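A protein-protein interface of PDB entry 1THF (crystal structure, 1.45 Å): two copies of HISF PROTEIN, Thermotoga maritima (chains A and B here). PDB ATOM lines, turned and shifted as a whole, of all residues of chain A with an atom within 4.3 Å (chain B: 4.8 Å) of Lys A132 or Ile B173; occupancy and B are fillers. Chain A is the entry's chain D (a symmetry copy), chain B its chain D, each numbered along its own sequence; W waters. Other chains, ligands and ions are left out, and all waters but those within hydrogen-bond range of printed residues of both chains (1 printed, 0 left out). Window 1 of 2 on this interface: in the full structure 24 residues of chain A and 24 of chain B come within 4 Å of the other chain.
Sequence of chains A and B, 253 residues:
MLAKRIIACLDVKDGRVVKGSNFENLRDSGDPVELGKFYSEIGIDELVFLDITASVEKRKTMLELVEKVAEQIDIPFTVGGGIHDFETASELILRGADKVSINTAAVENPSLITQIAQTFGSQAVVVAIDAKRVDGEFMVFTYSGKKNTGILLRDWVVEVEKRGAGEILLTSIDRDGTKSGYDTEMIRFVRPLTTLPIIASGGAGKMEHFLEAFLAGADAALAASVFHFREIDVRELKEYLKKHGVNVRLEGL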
ATOM      1  N   ALA A 131      -6.973  20.557 -15.546  1.00  0.00           N
ATOM      2  CA  ALA A 131      -8.284  21.097 -15.183  1.00  0.00           C
ATOM      3  C   ALA A 131      -9.359  20.691 -16.173  1.00  0.00           C
ATOM      4  O   ALA A 131      -9.097  20.288 -17.314  1.00  0.00           O
ATOM      5  CB  ALA A 131      -8.210  22.624 -15.147  1.00  0.00           C
ATOM      6  N   LYS A 132     -10.597  20.774 -15.691  1.00  0.00           N
ATOM      7  CA  LYS A 132     -11.794  20.512 -16.463  1.00  0.00           C
ATOM      8  C   LYS A 132     -12.860  21.535 -16.042  1.00  0.00           C
ATOM      9  O   LYS A 132     -12.813  22.004 -14.903  1.00  0.00           O
ATOM     10  CB  LYS A 132     -12.429  19.132 -16.232  1.00  0.00           C
ATOM     11  CG  LYS A 132     -11.495  17.939 -16.364  1.00  0.00           C
ATOM     12  CD  LYS A 132     -12.301  16.641 -16.367  1.00  0.00           C
ATOM     13  CE  LYS A 132     -11.403  15.429 -16.583  1.00  0.00           C
ATOM     14  NZ  LYS A 132     -12.075  14.466 -17.512  1.00  0.00           N
ATOM     15  N   ARG A 133     -13.794  21.798 -16.957  1.00  0.00           N
ATOM     16  CA  ARG A 133     -14.915  22.684 -16.610  1.00  0.00           C
ATOM     17  C   ARG A 133     -16.003  21.793 -16.012  1.00  0.00           C
ATOM     18  O   ARG A 133     -16.462  20.846 -16.648  1.00  0.00           O
ATOM     19  CB  ARG A 133     -15.375  23.456 -17.836  1.00  0.00           C
ATOM     20  CG  ARG A 133     -16.147  24.728 -17.482  1.00  0.00           C
ATOM     21  CD  ARG A 133     -16.345  25.577 -18.747  1.00  0.00           C
ATOM     22  NE  ARG A 133     -17.353  24.934 -19.584  1.00  0.00           N
ATOM     23  CZ  ARG A 133     -17.657  25.210 -20.843  1.00  0.00           C
ATOM     24  NH1 ARG A 133     -17.041  26.163 -21.529  1.00  0.00           N
ATOM     25  NH2 ARG A 133     -18.618  24.514 -21.448  1.00  0.00           N
ATOM     26  N   VAL A 134     -16.314  22.016 -14.749  1.00  0.00           N
ATOM     27  CA  VAL A 134     -17.285  21.225 -13.988  1.00  0.00           C
ATOM     28  C   VAL A 134     -18.497  22.098 -13.725  1.00  0.00           C
ATOM     29  O   VAL A 134     -18.432  23.070 -12.968  1.00  0.00           O
ATOM     30  CB  VAL A 134     -16.660  20.752 -12.663  1.00  0.00           C
ATOM     31  CG1 VAL A 134     -17.647  19.892 -11.879  1.00  0.00           C
ATOM     32  CG2 VAL A 134     -15.349  20.007 -12.932  1.00  0.00           C
ATOM     33  N   GLU A 137     -17.596  25.757 -13.976  1.00  0.00           N
ATOM     34  CA  GLU A 137     -16.478  26.253 -13.185  1.00  0.00           C
ATOM     35  C   GLU A 137     -15.233  25.393 -13.408  1.00  0.00           C
ATOM     36  O   GLU A 137     -15.273  24.165 -13.314  1.00  0.00           O
ATOM     37  CB  GLU A 137     -16.775  26.243 -11.675  1.00  0.00           C
ATOM     38  CG  GLU A 137     -17.914  27.191 -11.297  1.00  0.00           C
ATOM     39  CD  GLU A 137     -18.167  27.162  -9.801  1.00  0.00           C
ATOM     40  OE1 GLU A 137     -18.943  26.275  -9.400  1.00  0.00           O
ATOM     41  OE2 GLU A 137     -17.587  27.982  -9.067  1.00  0.00           O
ATOM     42  N   PHE A 138     -14.106  26.060 -13.695  1.00  0.00           N
ATOM     43  CA  PHE A 138     -12.853  25.300 -13.873  1.00  0.00           C
ATOM     44  C   PHE A 138     -12.354  24.767 -12.538  1.00  0.00           C
ATOM     45  O   PHE A 138     -12.181  25.526 -11.581  1.00  0.00           O
ATOM     46  CB  PHE A 138     -11.803  26.166 -14.552  1.00  0.00           C
ATOM     47  CG  PHE A 138     -12.044  26.452 -16.009  1.00  0.00           C
ATOM     48  CD1 PHE A 138     -11.989  25.454 -16.971  1.00  0.00           C
ATOM     49  CD2 PHE A 138     -12.292  27.744 -16.436  1.00  0.00           C
ATOM     50  CE1 PHE A 138     -12.200  25.729 -18.310  1.00  0.00           C
ATOM     51  CE2 PHE A 138     -12.508  28.031 -17.772  1.00  0.00           C
ATOM     52  CZ  PHE A 138     -12.457  27.020 -18.709  1.00  0.00           C
ATOM     53  N   MET A 139     -12.165  23.451 -12.447  1.00  0.00           N
ATOM     54  CA  MET A 139     -11.680  22.783 -11.257  1.00  0.00           C
ATOM     55  C   MET A 139     -10.392  22.003 -11.510  1.00  0.00           C
ATOM     56  O   MET A 139     -10.143  21.531 -12.628  1.00  0.00           O
ATOM     57  CB  MET A 139     -12.729  21.829 -10.680  1.00  0.00           C
ATOM     58  CG  MET A 139     -14.157  22.333 -10.601  1.00  0.00           C
ATOM     59  SD  MET A 139     -15.097  21.662  -9.201  1.00  0.00           S
ATOM     60  CE  MET A 139     -16.505  22.765  -9.180  1.00  0.00           C
ATOM     61  N   PHE A 141      -7.965  18.831 -11.143  1.00  0.00           N
ATOM     62  CA  PHE A 141      -8.018  17.385 -11.056  1.00  0.00           C
ATOM     63  C   PHE A 141      -6.628  16.810 -10.822  1.00  0.00           C
ATOM     64  O   PHE A 141      -5.656  17.238 -11.435  1.00  0.00           O
ATOM     65  CB  PHE A 141      -8.593  16.780 -12.342  1.00  0.00           C
ATOM     66  CG  PHE A 141     -10.088  16.899 -12.431  1.00  0.00           C
ATOM     67  CD1 PHE A 141     -10.717  18.125 -12.610  1.00  0.00           C
ATOM     68  CD2 PHE A 141     -10.864  15.755 -12.321  1.00  0.00           C
ATOM     69  CE1 PHE A 141     -12.095  18.219 -12.673  1.00  0.00           C
ATOM     70  CE2 PHE A 141     -12.244  15.846 -12.394  1.00  0.00           C
ATOM     71  CZ  PHE A 141     -12.866  17.070 -12.574  1.00  0.00           C
ATOM     72  N   GLY A 145      -6.306  12.888 -13.811  1.00  0.00           N
ATOM     73  CA  GLY A 145      -7.668  13.273 -14.087  1.00  0.00           C
ATOM     74  C   GLY A 145      -8.771  12.472 -13.453  1.00  0.00           C
ATOM     75  O   GLY A 145      -9.949  12.616 -13.807  1.00  0.00           O
ATOM     76  N   ILE A 173      -7.580  18.394 -19.871  1.00  0.00           N
ATOM     77  CA  ILE A 173      -7.756  16.956 -20.007  1.00  0.00           C
ATOM     78  C   ILE A 173      -8.771  16.626 -21.095  1.00  0.00           C
ATOM     79  O   ILE A 173      -8.562  15.720 -21.909  1.00  0.00           O
ATOM     80  CB  ILE A 173      -8.247  16.349 -18.669  1.00  0.00           C
ATOM     81  CG1 ILE A 173      -7.176  16.518 -17.581  1.00  0.00           C
ATOM     82  CG2 ILE A 173      -8.636  14.887 -18.847  1.00  0.00           C
ATOM     83  CD1 ILE A 173      -7.720  16.261 -16.176  1.00  0.00           C
ATOM     84  N   ASP A 174      -9.857  17.389 -21.181  1.00  0.00           N
ATOM     85  CA  ASP A 174     -10.946  17.100 -22.104  1.00  0.00           C
ATOM     86  C   ASP A 174     -10.643  17.404 -23.558  1.00  0.00           C
ATOM     87  O   ASP A 174     -11.429  17.002 -24.433  1.00  0.00           O
ATOM     88  CB  ASP A 174     -12.207  17.802 -21.588  1.00  0.00           C
ATOM     89  CG  ASP A 174     -12.618  17.305 -20.216  1.00  0.00           C
ATOM     90  OD1 ASP A 174     -12.202  16.204 -19.814  1.00  0.00           O
ATOM     91  OD2 ASP A 174     -13.365  18.028 -19.501  1.00  0.00           O
ATOM     92  N   ASP B 130     -11.448   3.162 -22.486  1.00  0.00           N
ATOM     93  CA  ASP B 130     -11.431   4.618 -22.402  1.00  0.00           C
ATOM     94  C   ASP B 130     -11.281   5.156 -23.826  1.00  0.00           C
ATOM     95  O   ASP B 130     -10.344   4.743 -24.520  1.00  0.00           O
ATOM     96  CB  ASP B 130     -10.262   5.127 -21.581  1.00  0.00           C
ATOM     97  CG  ASP B 130     -10.316   4.761 -20.115  1.00  0.00           C
ATOM     98  OD1 ASP B 130     -11.353   4.300 -19.608  1.00  0.00           O
ATOM     99  OD2 ASP B 130      -9.255   4.942 -19.463  1.00  0.00           O
ATOM    100  N   ALA B 131     -12.190   6.012 -24.231  1.00  0.00           N
ATOM    101  CA  ALA B 131     -12.132   6.524 -25.602  1.00  0.00           C
ATOM    102  C   ALA B 131     -12.360   8.022 -25.658  1.00  0.00           C
ATOM    103  O   ALA B 131     -12.892   8.651 -24.735  1.00  0.00           O
ATOM    104  CB  ALA B 131     -13.209   5.837 -26.443  1.00  0.00           C
ATOM    105  N   LYS B 132     -11.905   8.596 -26.770  1.00  0.00           N
ATOM    106  CA  LYS B 132     -12.069   9.998 -27.091  1.00  0.00           C
ATOM    107  C   LYS B 132     -12.352  10.107 -28.597  1.00  0.00           C
ATOM    108  O   LYS B 132     -11.915   9.232 -29.347  1.00  0.00           O
ATOM    109  CB  LYS B 132     -10.831  10.873 -26.838  1.00  0.00           C
ATOM    110  CG  LYS B 132     -10.208  10.761 -25.455  1.00  0.00           C
ATOM    111  CD  LYS B 132      -9.164  11.859 -25.261  1.00  0.00           C
ATOM    112  CE  LYS B 132      -8.580  11.828 -23.853  1.00  0.00           C
ATOM    113  NZ  LYS B 132      -8.428  13.228 -23.342  1.00  0.00           N
ATOM    114  N   PHE B 141      -7.797   4.887 -25.901  1.00  0.00           N
ATOM    115  CA  PHE B 141      -6.697   5.455 -25.147  1.00  0.00           C
ATOM    116  C   PHE B 141      -6.333   4.559 -23.972  1.00  0.00           C
ATOM    117  O   PHE B 141      -7.202   4.045 -23.276  1.00  0.00           O
ATOM    118  CB  PHE B 141      -7.060   6.847 -24.615  1.00  0.00           C
ATOM    119  CG  PHE B 141      -6.984   7.917 -25.666  1.00  0.00           C
ATOM    120  CD1 PHE B 141      -7.888   7.977 -26.719  1.00  0.00           C
ATOM    121  CD2 PHE B 141      -5.976   8.868 -25.590  1.00  0.00           C
ATOM    122  CE1 PHE B 141      -7.793   8.959 -27.687  1.00  0.00           C
ATOM    123  CE2 PHE B 141      -5.886   9.858 -26.553  1.00  0.00           C
ATOM    124  CZ  PHE B 141      -6.791   9.914 -27.601  1.00  0.00           C
ATOM    125  N   GLY B 145      -5.626   7.618 -20.155  1.00  0.00           N
ATOM    126  CA  GLY B 145      -5.887   8.595 -21.184  1.00  0.00           C
ATOM    127  C   GLY B 145      -4.718   9.340 -21.764  1.00  0.00           C
ATOM    128  O   GLY B 145      -4.887  10.326 -22.494  1.00  0.00           O
ATOM    129  N   THR B 171     -15.843   4.314 -20.909  1.00  0.00           N
ATOM    130  CA  THR B 171     -15.626   5.625 -20.322  1.00  0.00           C
ATOM    131  C   THR B 171     -15.299   6.685 -21.356  1.00  0.00           C
ATOM    132  O   THR B 171     -14.393   6.519 -22.172  1.00  0.00           O
ATOM    133  CB  THR B 171     -14.453   5.610 -19.310  1.00  0.00           C
ATOM    134  OG1 THR B 171     -14.781   4.681 -18.264  1.00  0.00           O
ATOM    135  CG2 THR B 171     -14.232   6.971 -18.664  1.00  0.00           C
ATOM    136  N   SER B 172     -16.011   7.797 -21.279  1.00  0.00           N
ATOM    137  CA  SER B 172     -15.692   8.948 -22.117  1.00  0.00           C
ATOM    138  C   SER B 172     -14.824   9.846 -21.238  1.00  0.00           C
ATOM    139  O   SER B 172     -15.305  10.579 -20.367  1.00  0.00           O
ATOM    140  CB  SER B 172     -16.943   9.647 -22.606  1.00  0.00           C
ATOM    141  OG  SER B 172     -16.570  10.789 -23.386  1.00  0.00           O
ATOM    142  N   ILE B 173     -13.515   9.796 -21.459  1.00  0.00           N
ATOM    143  CA  ILE B 173     -12.555  10.576 -20.693  1.00  0.00           C
ATOM    144  C   ILE B 173     -12.912  12.058 -20.708  1.00  0.00           C
ATOM    145  O   ILE B 173     -12.854  12.739 -19.679  1.00  0.00           O
ATOM    146  CB  ILE B 173     -11.133  10.403 -21.283  1.00  0.00           C
ATOM    147  CG1 ILE B 173     -10.668   8.946 -21.137  1.00  0.00           C
ATOM    148  CG2 ILE B 173     -10.153  11.369 -20.630  1.00  0.00           C
ATOM    149  CD1 ILE B 173      -9.442   8.631 -21.993  1.00  0.00           C
ATOM    150  N   ASP B 174     -13.355  12.576 -21.850  1.00  0.00           N
ATOM    151  CA  ASP B 174     -13.618  14.000 -22.015  1.00  0.00           C
ATOM    152  C   ASP B 174     -14.876  14.495 -21.327  1.00  0.00           C
ATOM    153  O   ASP B 174     -15.070  15.719 -21.240  1.00  0.00           O
ATOM    154  CB  ASP B 174     -13.579  14.322 -23.512  1.00  0.00           C
ATOM    155  CG  ASP B 174     -12.225  14.027 -24.126  1.00  0.00           C
ATOM    156  OD1 ASP B 174     -11.225  13.942 -23.390  1.00  0.00           O
ATOM    157  OD2 ASP B 174     -12.140  13.860 -25.374  1.00  0.00           O
ATOM    158  N   ARG B 175     -15.715  13.577 -20.826  1.00  0.00           N
ATOM    159  CA  ARG B 175     -16.857  13.981 -20.026  1.00  0.00           C
ATOM    160  C   ARG B 175     -16.674  13.616 -18.557  1.00  0.00           C
ATOM    161  O   ARG B 175     -17.380  14.115 -17.681  1.00  0.00           O
ATOM    162  CB  ARG B 175     -18.143  13.267 -20.465  1.00  0.00           C
ATOM    163  CG  ARG B 175     -18.540  13.406 -21.910  1.00  0.00           C
ATOM    164  CD  ARG B 175     -18.708  14.856 -22.317  1.00  0.00           C
ATOM    165  NE  ARG B 175     -19.525  15.023 -23.507  1.00  0.00           N
ATOM    166  CZ  ARG B 175     -20.846  14.919 -23.556  1.00  0.00           C
ATOM    167  NH1 ARG B 175     -21.542  14.650 -22.459  1.00  0.00           N
ATOM    168  NH2 ARG B 175     -21.475  15.092 -24.708  1.00  0.00           N
ATOM    169  N   ASP B 176     -15.743  12.719 -18.256  1.00  0.00           N
ATOM    170  CA  ASP B 176     -15.517  12.251 -16.888  1.00  0.00           C
ATOM    171  C   ASP B 176     -15.276  13.373 -15.909  1.00  0.00           C
ATOM    172  O   ASP B 176     -14.413  14.235 -16.096  1.00  0.00           O
ATOM    173  CB  ASP B 176     -14.341  11.273 -16.903  1.00  0.00           C
ATOM    174  CG  ASP B 176     -14.198  10.379 -15.701  1.00  0.00           C
ATOM    175  OD1 ASP B 176     -14.858  10.564 -14.667  1.00  0.00           O
ATOM    176  OD2 ASP B 176     -13.365   9.432 -15.765  1.00  0.00           O
ATOM    177  N   THR B 178     -17.113  15.982 -15.361  1.00  0.00           N
ATOM    178  CA  THR B 178     -17.602  17.288 -15.776  1.00  0.00           C
ATOM    179  C   THR B 178     -19.016  17.584 -15.307  1.00  0.00           C
ATOM    180  O   THR B 178     -19.454  18.738 -15.347  1.00  0.00           O
ATOM    181  CB  THR B 178     -17.567  17.491 -17.307  1.00  0.00           C
ATOM    182  OG1 THR B 178     -18.500  16.570 -17.906  1.00  0.00           O
ATOM    183  CG2 THR B 178     -16.158  17.293 -17.837  1.00  0.00           C
HETATM  184  O   HOH W   1     -13.067  12.484 -13.114  1.00  0.00           O
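Lys A132 touches Ile B173, and with the chains exchanged Ile A173 touches Lys B132. Ile A173 touches Asp B174, and with the chains exchanged Asp A174 touches Ile B173. Asp A174 touches its own counterpart, Asp B174. 6 positions are printed for both chains. Of the 9 pairs that touch across the chains among the printed residues, 5 have their exchanged pair printed and touching as well.
O of Ile A173 sits at hydrogen-bond distance from NZ of Lys B132 (2.9 Å). The backbone carbonyl oxygen (O) of Asp B176 sits at hydrogen-bond distance from the side-chain amino group (NZ) of Lys A132. The backbone carbonyl oxygen (O) of Ile B173 sits at hydrogen-bond distance from the side-chain amino group (NZ) of Lys A132 (2.9 Å). OD1 of Asp B174 sits close to O of Asp A174 (3.2 Å).
Along chain B the printed residues that touch a printed residue of chain A span positions 132 to 178. Of the 11 printed residues of chain A, 5 touch a printed residue of chain B. Among the printed residues, no Asp or Glu carboxylate lies within 4 Å of a Lys or Arg side-chain nitrogen of the other chain.
The side-chain carboxylate (OD1) of Asp B174 is in salt-bridge range of the side-chain amino group (NZ) of Lys B132, 2.9 Å away. The backbone carbonyl oxygen (O) of Arg B175 lies within hydrogen-bond range of the side-chain hydroxyl (OG1) of Thr B178, at 2.7 Å. O of Lys A132 lies within hydrogen-bond range of N of Met A139 (2.9 Å). NZ of Lys A132 is in salt-bridge range of OD1 of Asp A174 (2.9 Å).
Thr B178 touches Arg A133. Val A134 touches Thr B178. Asp B174 touches Ile A173. OD1 of Asp A174 touches O of Ile B173, at 3.5 Å. OD2 of Asp A174 touches CG2 of Thr B178 (3.3 Å).
Water W1 bridges the side-chain carboxylate (OD1) of Asp B176 and the backbone carbonyl oxygen (O) of Gly A145.
Of the printed residues of chain B, Lys A132 touches Ile B173 and Asp B176. Printed residues of chain B within 4 Å of Arg A133: Thr B178. Printed residues of chain B within 4 Å of Asp A174: Ile B173, Asp B174 and Thr B178. Ile B173 touches just these residues of chain A: Lys A132 (2.9 Å) and Asp A174 (3.5 Å). The nearest printed residue of chain A that does not touch Thr B178 is Lys A132 (4.2 Å).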
